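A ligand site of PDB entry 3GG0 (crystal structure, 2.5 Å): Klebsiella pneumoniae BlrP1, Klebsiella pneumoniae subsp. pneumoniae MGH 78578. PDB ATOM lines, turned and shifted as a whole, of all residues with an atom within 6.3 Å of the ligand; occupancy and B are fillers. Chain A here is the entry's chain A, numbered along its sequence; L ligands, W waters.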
ATOM      1  N   TYR A  15      -5.194  20.727  -6.679  1.00  0.00           N
ATOM      2  CA  TYR A  15      -5.777  20.161  -5.462  1.00  0.00           C
ATOM      3  C   TYR A  15      -4.750  20.047  -4.349  1.00  0.00           C
ATOM      4  O   TYR A  15      -3.544  20.104  -4.593  1.00  0.00           O
ATOM      5  CB  TYR A  15      -6.409  18.785  -5.750  1.00  0.00           C
ATOM      6  CG  TYR A  15      -5.398  17.682  -6.004  1.00  0.00           C
ATOM      7  CD1 TYR A  15      -4.792  17.009  -4.937  1.00  0.00           C
ATOM      8  CD2 TYR A  15      -5.044  17.318  -7.289  1.00  0.00           C
ATOM      9  CE1 TYR A  15      -3.854  16.017  -5.161  1.00  0.00           C
ATOM     10  CE2 TYR A  15      -4.113  16.324  -7.530  1.00  0.00           C
ATOM     11  CZ  TYR A  15      -3.519  15.677  -6.459  1.00  0.00           C
ATOM     12  OH  TYR A  15      -2.590  14.689  -6.687  1.00  0.00           O
ATOM     13  N   SER A  17      -3.997  17.363  -0.831  1.00  0.00           N
ATOM     14  CA  SER A  17      -4.367  16.120  -0.165  1.00  0.00           C
ATOM     15  C   SER A  17      -3.432  15.819   0.994  1.00  0.00           C
ATOM     16  O   SER A  17      -2.441  16.520   1.191  1.00  0.00           O
ATOM     17  CB  SER A  17      -4.360  14.957  -1.159  1.00  0.00           C
ATOM     18  OG  SER A  17      -3.052  14.743  -1.671  1.00  0.00           O
ATOM     19  N   VAL A  26       5.204   6.591   1.468  1.00  0.00           N
ATOM     20  CA  VAL A  26       5.098   6.329   0.042  1.00  0.00           C
ATOM     21  C   VAL A  26       6.406   6.690  -0.662  1.00  0.00           C
ATOM     22  O   VAL A  26       6.990   7.745  -0.406  1.00  0.00           O
ATOM     23  CB  VAL A  26       3.921   7.129  -0.592  1.00  0.00           C
ATOM     24  CG1 VAL A  26       3.855   6.897  -2.092  1.00  0.00           C
ATOM     25  CG2 VAL A  26       2.603   6.745   0.075  1.00  0.00           C
ATOM     26  N   LEU A  28       8.051   8.334  -3.146  1.00  0.00           N
ATOM     27  CA  LEU A  28       7.604   9.436  -3.984  1.00  0.00           C
ATOM     28  C   LEU A  28       8.471   9.642  -5.207  1.00  0.00           C
ATOM     29  O   LEU A  28       7.991  10.118  -6.238  1.00  0.00           O
ATOM     30  CB  LEU A  28       7.526  10.733  -3.178  1.00  0.00           C
ATOM     31  CG  LEU A  28       6.286  10.911  -2.333  1.00  0.00           C
ATOM     32  CD1 LEU A  28       6.402  12.152  -1.460  1.00  0.00           C
ATOM     33  CD2 LEU A  28       5.037  10.988  -3.218  1.00  0.00           C
ATOM     34  N   LEU A  31       6.907   7.470  -7.575  1.00  0.00           N
ATOM     35  CA  LEU A  31       5.619   8.053  -7.946  1.00  0.00           C
ATOM     36  C   LEU A  31       5.801   9.157  -8.969  1.00  0.00           C
ATOM     37  O   LEU A  31       5.102   9.181  -9.982  1.00  0.00           O
ATOM     38  CB  LEU A  31       4.907   8.611  -6.699  1.00  0.00           C
ATOM     39  CG  LEU A  31       3.399   8.903  -6.786  1.00  0.00           C
ATOM     40  CD1 LEU A  31       2.757   8.819  -5.410  1.00  0.00           C
ATOM     41  CD2 LEU A  31       3.100  10.259  -7.435  1.00  0.00           C
ATOM     42  N   ARG A  34       7.349   7.946 -12.476  1.00  0.00           N
ATOM     43  CA  ARG A  34       6.285   7.222 -13.174  1.00  0.00           C
ATOM     44  C   ARG A  34       5.200   8.186 -13.683  1.00  0.00           C
ATOM     45  O   ARG A  34       4.650   8.008 -14.770  1.00  0.00           O
ATOM     46  CB  ARG A  34       5.675   6.160 -12.262  1.00  0.00           C
ATOM     47  CG  ARG A  34       4.870   5.098 -12.971  1.00  0.00           C
ATOM     48  CD  ARG A  34       4.503   3.954 -12.036  1.00  0.00           C
ATOM     49  NE  ARG A  34       3.461   3.097 -12.608  1.00  0.00           N
ATOM     50  CZ  ARG A  34       3.702   2.043 -13.388  1.00  0.00           C
ATOM     51  NH1 ARG A  34       4.948   1.706 -13.683  1.00  0.00           N
ATOM     52  NH2 ARG A  34       2.688   1.321 -13.857  1.00  0.00           N
ATOM     53  N   ALA A  35       4.919   9.217 -12.885  1.00  0.00           N
ATOM     54  CA  ALA A  35       3.933  10.233 -13.238  1.00  0.00           C
ATOM     55  C   ALA A  35       4.404  11.093 -14.397  1.00  0.00           C
ATOM     56  O   ALA A  35       3.655  11.329 -15.341  1.00  0.00           O
ATOM     57  CB  ALA A  35       3.599  11.102 -12.029  1.00  0.00           C
ATOM     58  N   SER A  36       5.654  11.548 -14.317  1.00  0.00           N
ATOM     59  CA  SER A  36       6.223  12.408 -15.354  1.00  0.00           C
ATOM     60  C   SER A  36       6.303  11.658 -16.672  1.00  0.00           C
ATOM     61  O   SER A  36       6.041  12.224 -17.745  1.00  0.00           O
ATOM     62  CB  SER A  36       7.617  12.896 -14.936  1.00  0.00           C
ATOM     63  OG  SER A  36       7.980  14.070 -15.645  1.00  0.00           O
ATOM     64  N   LYS A  38       4.281   9.290 -17.576  1.00  0.00           N
ATOM     65  CA  LYS A  38       2.926   9.078 -18.069  1.00  0.00           C
ATOM     66  C   LYS A  38       2.263  10.380 -18.535  1.00  0.00           C
ATOM     67  O   LYS A  38       1.498  10.372 -19.499  1.00  0.00           O
ATOM     68  CB  LYS A  38       2.076   8.384 -16.994  1.00  0.00           C
ATOM     69  CG  LYS A  38       0.856   7.665 -17.533  1.00  0.00           C
ATOM     70  CD  LYS A  38       0.096   6.977 -16.408  1.00  0.00           C
ATOM     71  CE  LYS A  38      -1.309   6.628 -16.838  1.00  0.00           C
ATOM     72  NZ  LYS A  38      -2.202   6.377 -15.670  1.00  0.00           N
ATOM     73  N   ASN A  39       2.574  11.481 -17.854  1.00  0.00           N
ATOM     74  CA  ASN A  39       1.910  12.768 -18.099  1.00  0.00           C
ATOM     75  C   ASN A  39       2.254  13.385 -19.457  1.00  0.00           C
ATOM     76  O   ASN A  39       1.377  13.861 -20.170  1.00  0.00           O
ATOM     77  CB  ASN A  39       2.234  13.761 -16.988  1.00  0.00           C
ATOM     78  CG  ASN A  39       1.479  13.467 -15.706  1.00  0.00           C
ATOM     79  OD1 ASN A  39       0.645  12.570 -15.647  1.00  0.00           O
ATOM     80  ND2 ASN A  39       1.768  14.238 -14.665  1.00  0.00           N
ATOM     81  N   ILE A  44       0.118  16.295 -20.440  1.00  0.00           N
ATOM     82  CA  ILE A  44      -0.120  16.745 -19.072  1.00  0.00           C
ATOM     83  C   ILE A  44       1.188  17.219 -18.453  1.00  0.00           C
ATOM     84  O   ILE A  44       2.211  16.535 -18.534  1.00  0.00           O
ATOM     85  CB  ILE A  44      -0.753  15.637 -18.191  1.00  0.00           C
ATOM     86  CG1 ILE A  44      -2.019  15.091 -18.829  1.00  0.00           C
ATOM     87  CG2 ILE A  44      -1.052  16.162 -16.777  1.00  0.00           C
ATOM     88  CD1 ILE A  44      -2.573  13.852 -18.161  1.00  0.00           C
ATOM     89  N   LEU A  48       4.454  18.768  -8.185  1.00  0.00           N
ATOM     90  CA  LEU A  48       3.955  18.245  -6.919  1.00  0.00           C
ATOM     91  C   LEU A  48       4.671  18.925  -5.763  1.00  0.00           C
ATOM     92  O   LEU A  48       5.880  19.114  -5.797  1.00  0.00           O
ATOM     93  CB  LEU A  48       4.160  16.733  -6.859  1.00  0.00           C
ATOM     94  CG  LEU A  48       3.515  16.001  -5.692  1.00  0.00           C
ATOM     95  CD1 LEU A  48       2.039  16.310  -5.612  1.00  0.00           C
ATOM     96  CD2 LEU A  48       3.746  14.505  -5.827  1.00  0.00           C
ATOM     97  N   PHE A  55       0.081  16.874   0.269  1.00  0.00           N
ATOM     98  CA  PHE A  55       0.466  17.095  -1.116  1.00  0.00           C
ATOM     99  C   PHE A  55      -0.224  18.324  -1.672  1.00  0.00           C
ATOM    100  O   PHE A  55      -1.274  18.731  -1.176  1.00  0.00           O
ATOM    101  CB  PHE A  55       0.133  15.889  -1.981  1.00  0.00           C
ATOM    102  CG  PHE A  55       0.847  14.646  -1.585  1.00  0.00           C
ATOM    103  CD1 PHE A  55       2.217  14.520  -1.815  1.00  0.00           C
ATOM    104  CD2 PHE A  55       0.167  13.601  -0.990  1.00  0.00           C
ATOM    105  CE1 PHE A  55       2.879  13.366  -1.447  1.00  0.00           C
ATOM    106  CE2 PHE A  55       0.829  12.448  -0.621  1.00  0.00           C
ATOM    107  CZ  PHE A  55       2.193  12.334  -0.850  1.00  0.00           C
ATOM    108  N   GLN A  57      -0.758  19.607  -5.772  1.00  0.00           N
ATOM    109  CA  GLN A  57      -0.434  19.305  -7.156  1.00  0.00           C
ATOM    110  C   GLN A  57      -1.092  20.244  -8.145  1.00  0.00           C
ATOM    111  O   GLN A  57      -2.275  20.552  -8.044  1.00  0.00           O
ATOM    112  CB  GLN A  57      -0.788  17.848  -7.486  1.00  0.00           C
ATOM    113  CG  GLN A  57      -0.141  17.350  -8.767  1.00  0.00           C
ATOM    114  CD  GLN A  57      -0.355  15.870  -8.997  1.00  0.00           C
ATOM    115  OE1 GLN A  57      -1.361  15.301  -8.588  1.00  0.00           O
ATOM    116  NE2 GLN A  57       0.603  15.242  -9.665  1.00  0.00           N
ATOM    117  N   LEU A  59      -1.906  20.640 -12.239  1.00  0.00           N
ATOM    118  CA  LEU A  59      -2.029  19.856 -13.450  1.00  0.00           C
ATOM    119  C   LEU A  59      -2.468  20.713 -14.620  1.00  0.00           C
ATOM    120  O   LEU A  59      -3.406  21.488 -14.493  1.00  0.00           O
ATOM    121  CB  LEU A  59      -3.009  18.695 -13.261  1.00  0.00           C
ATOM    122  CG  LEU A  59      -2.594  17.567 -12.294  1.00  0.00           C
ATOM    123  CD1 LEU A  59      -3.737  16.579 -12.098  1.00  0.00           C
ATOM    124  CD2 LEU A  59      -1.339  16.857 -12.792  1.00  0.00           C
ATOM    125  N   LEU A  69      -7.429  11.755 -15.418  1.00  0.00           N
ATOM    126  CA  LEU A  69      -6.287  11.608 -14.520  1.00  0.00           C
ATOM    127  C   LEU A  69      -6.691  11.820 -13.058  1.00  0.00           C
ATOM    128  O   LEU A  69      -6.229  11.107 -12.166  1.00  0.00           O
ATOM    129  CB  LEU A  69      -5.160  12.568 -14.915  1.00  0.00           C
ATOM    130  CG  LEU A  69      -3.920  12.549 -14.024  1.00  0.00           C
ATOM    131  CD1 LEU A  69      -3.237  11.193 -14.071  1.00  0.00           C
ATOM    132  CD2 LEU A  69      -2.936  13.653 -14.412  1.00  0.00           C
ATOM    133  N   GLU A  72      -8.428   8.888 -11.310  1.00  0.00           N
ATOM    134  CA  GLU A  72      -7.410   7.965 -10.820  1.00  0.00           C
ATOM    135  C   GLU A  72      -6.749   8.483  -9.553  1.00  0.00           C
ATOM    136  O   GLU A  72      -6.567   7.742  -8.591  1.00  0.00           O
ATOM    137  CB  GLU A  72      -6.350   7.723 -11.903  1.00  0.00           C
ATOM    138  CG  GLU A  72      -6.778   6.747 -12.991  1.00  0.00           C
ATOM    139  CD  GLU A  72      -5.622   6.334 -13.876  1.00  0.00           C
ATOM    140  OE1 GLU A  72      -4.871   7.223 -14.352  1.00  0.00           O
ATOM    141  OE2 GLU A  72      -5.457   5.114 -14.116  1.00  0.00           O
ATOM    142  N   ILE A  73      -6.420   9.774  -9.552  1.00  0.00           N
ATOM    143  CA  ILE A  73      -5.775  10.413  -8.413  1.00  0.00           C
ATOM    144  C   ILE A  73      -6.684  10.446  -7.177  1.00  0.00           C
ATOM    145  O   ILE A  73      -6.234  10.196  -6.049  1.00  0.00           O
ATOM    146  CB  ILE A  73      -5.256  11.830  -8.766  1.00  0.00           C
ATOM    147  CG1 ILE A  73      -3.934  11.730  -9.537  1.00  0.00           C
ATOM    148  CG2 ILE A  73      -5.063  12.674  -7.507  1.00  0.00           C
ATOM    149  CD1 ILE A  73      -3.497  13.024 -10.160  1.00  0.00           C
ATOM    150  N   GLN A  74      -7.971  10.723  -7.394  1.00  0.00           N
ATOM    151  CA  GLN A  74      -8.971  10.741  -6.320  1.00  0.00           C
ATOM    152  C   GLN A  74      -9.062   9.397  -5.595  1.00  0.00           C
ATOM    153  O   GLN A  74      -9.220   9.350  -4.369  1.00  0.00           O
ATOM    154  CB  GLN A  74     -10.347  11.107  -6.870  1.00  0.00           C
ATOM    155  CG  GLN A  74     -10.654  12.585  -6.878  1.00  0.00           C
ATOM    156  CD  GLN A  74     -11.935  12.896  -7.615  1.00  0.00           C
ATOM    157  OE1 GLN A  74     -12.212  12.332  -8.676  1.00  0.00           O
ATOM    158  NE2 GLN A  74     -12.736  13.806  -7.053  1.00  0.00           N
ATOM    159  N   SER A  75      -8.992   8.313  -6.357  1.00  0.00           N
ATOM    160  CA  SER A  75      -9.213   6.978  -5.816  1.00  0.00           C
ATOM    161  C   SER A  75      -7.918   6.285  -5.377  1.00  0.00           C
ATOM    162  O   SER A  75      -7.940   5.117  -4.989  1.00  0.00           O
ATOM    163  CB  SER A  75      -9.962   6.110  -6.825  1.00  0.00           C
ATOM    164  OG  SER A  75     -11.277   6.599  -7.008  1.00  0.00           O
ATOM    165  N   ASP A  76      -6.809   7.018  -5.453  1.00  0.00           N
ATOM    166  CA  ASP A  76      -5.509   6.492  -5.041  1.00  0.00           C
ATOM    167  C   ASP A  76      -5.414   6.409  -3.517  1.00  0.00           C
ATOM    168  O   ASP A  76      -5.534   7.432  -2.830  1.00  0.00           O
ATOM    169  CB  ASP A  76      -4.383   7.361  -5.592  1.00  0.00           C
ATOM    170  CG  ASP A  76      -3.066   6.633  -5.681  1.00  0.00           C
ATOM    171  OD1 ASP A  76      -2.610   6.075  -4.659  1.00  0.00           O
ATOM    172  OD2 ASP A  76      -2.464   6.619  -6.770  1.00  0.00           O
ATOM    173  N   ARG A  78      -2.962   5.982  -1.652  1.00  0.00           N
ATOM    174  CA  ARG A  78      -1.708   6.517  -1.096  1.00  0.00           C
ATOM    175  C   ARG A  78      -1.883   7.912  -0.482  1.00  0.00           C
ATOM    176  O   ARG A  78      -0.999   8.403   0.222  1.00  0.00           O
ATOM    177  CB  ARG A  78      -0.609   6.522  -2.158  1.00  0.00           C
ATOM    178  CG  ARG A  78      -0.042   5.138  -2.480  1.00  0.00           C
ATOM    179  CD  ARG A  78       0.882   5.179  -3.690  1.00  0.00           C
ATOM    180  NE  ARG A  78       0.146   5.437  -4.918  1.00  0.00           N
ATOM    181  CZ  ARG A  78       0.712   5.587  -6.116  1.00  0.00           C
ATOM    182  NH1 ARG A  78      -0.043   5.821  -7.183  1.00  0.00           N
ATOM    183  NH2 ARG A  78       2.021   5.503  -6.243  1.00  0.00           N
ATOM    184  N   HIS A  79      -3.024   8.537  -0.748  1.00  0.00           N
ATOM    185  CA  HIS A  79      -3.419   9.737  -0.026  1.00  0.00           C
ATOM    186  C   HIS A  79      -4.910   9.788   0.255  1.00  0.00           C
ATOM    187  O   HIS A  79      -5.681   8.941  -0.219  1.00  0.00           O
ATOM    188  CB  HIS A  79      -2.942  11.017  -0.753  1.00  0.00           C
ATOM    189  CG  HIS A  79      -3.596  11.257  -2.077  1.00  0.00           C
ATOM    190  ND1 HIS A  79      -3.150  12.210  -2.962  1.00  0.00           N
ATOM    191  CD2 HIS A  79      -4.656  10.664  -2.673  1.00  0.00           C
ATOM    192  CE1 HIS A  79      -3.921  12.201  -4.049  1.00  0.00           C
ATOM    193  NE2 HIS A  79      -4.840  11.265  -3.895  1.00  0.00           N
ATOM    194  N   GLY A  99       6.485  17.116 -17.172  1.00  0.00           N
ATOM    195  CA  GLY A  99       5.408  16.140 -16.948  1.00  0.00           C
ATOM    196  C   GLY A  99       4.975  16.110 -15.501  1.00  0.00           C
ATOM    197  O   GLY A  99       3.798  16.337 -15.190  1.00  0.00           O
ATOM    198  N   MET A 100       5.922  15.836 -14.612  1.00  0.00           N
ATOM    199  CA  MET A 100       5.707  15.963 -13.180  1.00  0.00           C
ATOM    200  C   MET A 100       7.054  16.135 -12.480  1.00  0.00           C
ATOM    201  O   MET A 100       8.078  15.641 -12.953  1.00  0.00           O
ATOM    202  CB  MET A 100       4.972  14.739 -12.637  1.00  0.00           C
ATOM    203  CG  MET A 100       4.383  14.939 -11.228  1.00  0.00           C
ATOM    204  SD  MET A 100       3.699  16.595 -10.932  1.00  0.00           S
ATOM    205  CE  MET A 100       2.334  16.643 -12.092  1.00  0.00           C
HETATM  206  N1  LIG L   1      -0.454   9.604 -11.929  1.00  0.00           N
HETATM  207  C1  LIG L   1      -0.147  10.182 -13.131  1.00  0.00           C
HETATM  208  O1  LIG L   1      -0.244   9.505 -14.166  1.00  0.00           O
HETATM  209  N2  LIG L   1       0.250  11.499 -13.192  1.00  0.00           N
HETATM  210  C2  LIG L   1       0.347  12.239 -12.036  1.00  0.00           C
HETATM  211  O2  LIG L   1       0.619  13.431 -12.105  1.00  0.00           O
HETATM  212  C3  LIG L   1       0.040  11.650 -10.815  1.00  0.00           C
HETATM  213  N3  LIG L   1       0.133  12.387  -9.651  1.00  0.00           N
HETATM  214  C4  LIG L   1      -0.162  11.813  -8.442  1.00  0.00           C
HETATM  215  C5  LIG L   1      -0.052  12.566  -7.274  1.00  0.00           C
HETATM  216  C6  LIG L   1      -0.358  11.991  -6.036  1.00  0.00           C
HETATM  217  C7  LIG L   1      -0.049  12.758  -4.783  1.00  0.00           C
HETATM  218  C8  LIG L   1      -0.771  10.666  -5.973  1.00  0.00           C
HETATM  219  C9  LIG L   1      -0.822   9.966  -4.639  1.00  0.00           C
HETATM  220  C10 LIG L   1      -0.873   9.909  -7.139  1.00  0.00           C
HETATM  221  C11 LIG L   1      -0.569  10.476  -8.382  1.00  0.00           C
HETATM  222  N4  LIG L   1      -0.671   9.743  -9.549  1.00  0.00           N
HETATM  223  C12 LIG L   1      -0.359  10.325 -10.759  1.00  0.00           C
HETATM  224  C13 LIG L   1      -0.896   8.250  -9.491  1.00  0.00           C
HETATM  225  C14 LIG L   1      -2.319   7.909  -9.927  1.00  0.00           C
HETATM  226  O3  LIG L   1      -3.204   8.061  -8.835  1.00  0.00           O
HETATM  227  C15 LIG L   1      -2.402   6.470 -10.454  1.00  0.00           C
HETATM  228  O4  LIG L   1      -1.983   5.571  -9.455  1.00  0.00           O
HETATM  229  C16 LIG L   1      -1.539   6.257 -11.702  1.00  0.00           C
HETATM  230  O5  LIG L   1      -1.827   7.233 -12.674  1.00  0.00           O
HETATM  231  C17 LIG L   1      -1.796   4.875 -12.286  1.00  0.00           C
HETATM  232  O6  LIG L   1      -1.270   4.812 -13.590  1.00  0.00           O
HETATM  233  P1  LIG L   1      -0.709   3.423 -14.180  1.00  0.00           P
HETATM  234  O7  LIG L   1      -1.628   2.300 -13.705  1.00  0.00           O
HETATM  235  O8  LIG L   1      -0.715   3.483 -15.689  1.00  0.00           O
HETATM  236  O9  LIG L   1       0.689   3.187 -13.686  1.00  0.00           O
HETATM  237  O   HOH W   1      -2.256   1.621 -16.525  1.00  0.00           O
HETATM  238  O   HOH W   2       1.678   7.678 -13.094  1.00  0.00           O
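Water W2 bridges O1 of the ligand (2.9 Å) and O of Arg 34 (3.4 Å).
Merely in contact with the ligand: Tyr 15 (3.4 Å), Leu 69 (3.4 Å), Ala 35 (3.4 Å), Ile 73 (3.5 Å), His 79 (3.6 Å), Met 100 (3.6 Å), Leu 31 (3.8 Å) and Phe 55 (3.8 Å).
Hydrophobic or aromatic side chains that line the ligand: Leu 31, Ala 35, Phe 55, Leu 69, Ile 73, His 79 and Met 100.
Within 4 Å of the ligand: Tyr 15, Leu 31, Arg 34, Ala 35, Lys 38, Asn 39, Phe 55, Gln 57, Leu 69, Glu 72, Ile 73, Asp 76, Arg 78, His 79 and Met 100.
The nearest printed residue that does not touch the ligand is Leu 59 (4.01 Å).
An oxygen (O3) of the ligand is in hydrogen-bond range of the side-chain carboxylate (OD2) of Asp 76 (2.6 Å).
OD1 of Asn 39 sits at hydrogen-bond distance from N2 of the ligand (2.7 Å).
O9 of the ligand is in salt-bridge range of NH2 of Arg 34.
NZ of Lys 38 is in salt-bridge range of O8 of the ligand.
NE2 of Gln 57 is in hydrogen-bond range of N3 of the ligand (2.9 Å).
An oxygen (O4) of the ligand is in hydrogen-bond range of the guanidinium group (NH1) of Arg 78.
The backbone carbonyl oxygen (O) of Glu 72 is in hydrogen-bond range of an oxygen (O3) of the ligand.
OE1 of Glu 72 lies within hydrogen-bond range of O5 of the ligand (3.5 Å).
The guanidinium group of Arg 78 lies within salt-bridge range of the side-chain carboxylate of Asp 76.
The side-chain amino group of Lys 38 is in salt-bridge range of the side-chain carboxylate of Glu 72.
The backbone carbonyl oxygen (O) of Tyr 15 is in hydrogen-bond range of the backbone NH (N) of Gln 57 (3.1 Å).
SD of Met 100 lies close to NE2 of Gln 57 (3.6 Å).
The backbone carbonyl oxygen of Ile 73 is in hydrogen-bond range of a ring nitrogen (NE2) of His 79 (2.8 Å).
A ring nitrogen (ND1) of His 79 sits at hydrogen-bond distance from the side-chain hydroxyl of Ser 17, at 2.8 Å.
The backbone NH (N) of Met 100 lies within hydrogen-bond range of the side-chain hydroxyl (OG) of Ser 36 (2.9 Å).
The backbone NH (N) of Phe 55 lies within hydrogen-bond range of the backbone carbonyl oxygen (O) of Ser 17, at 2.7 Å.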
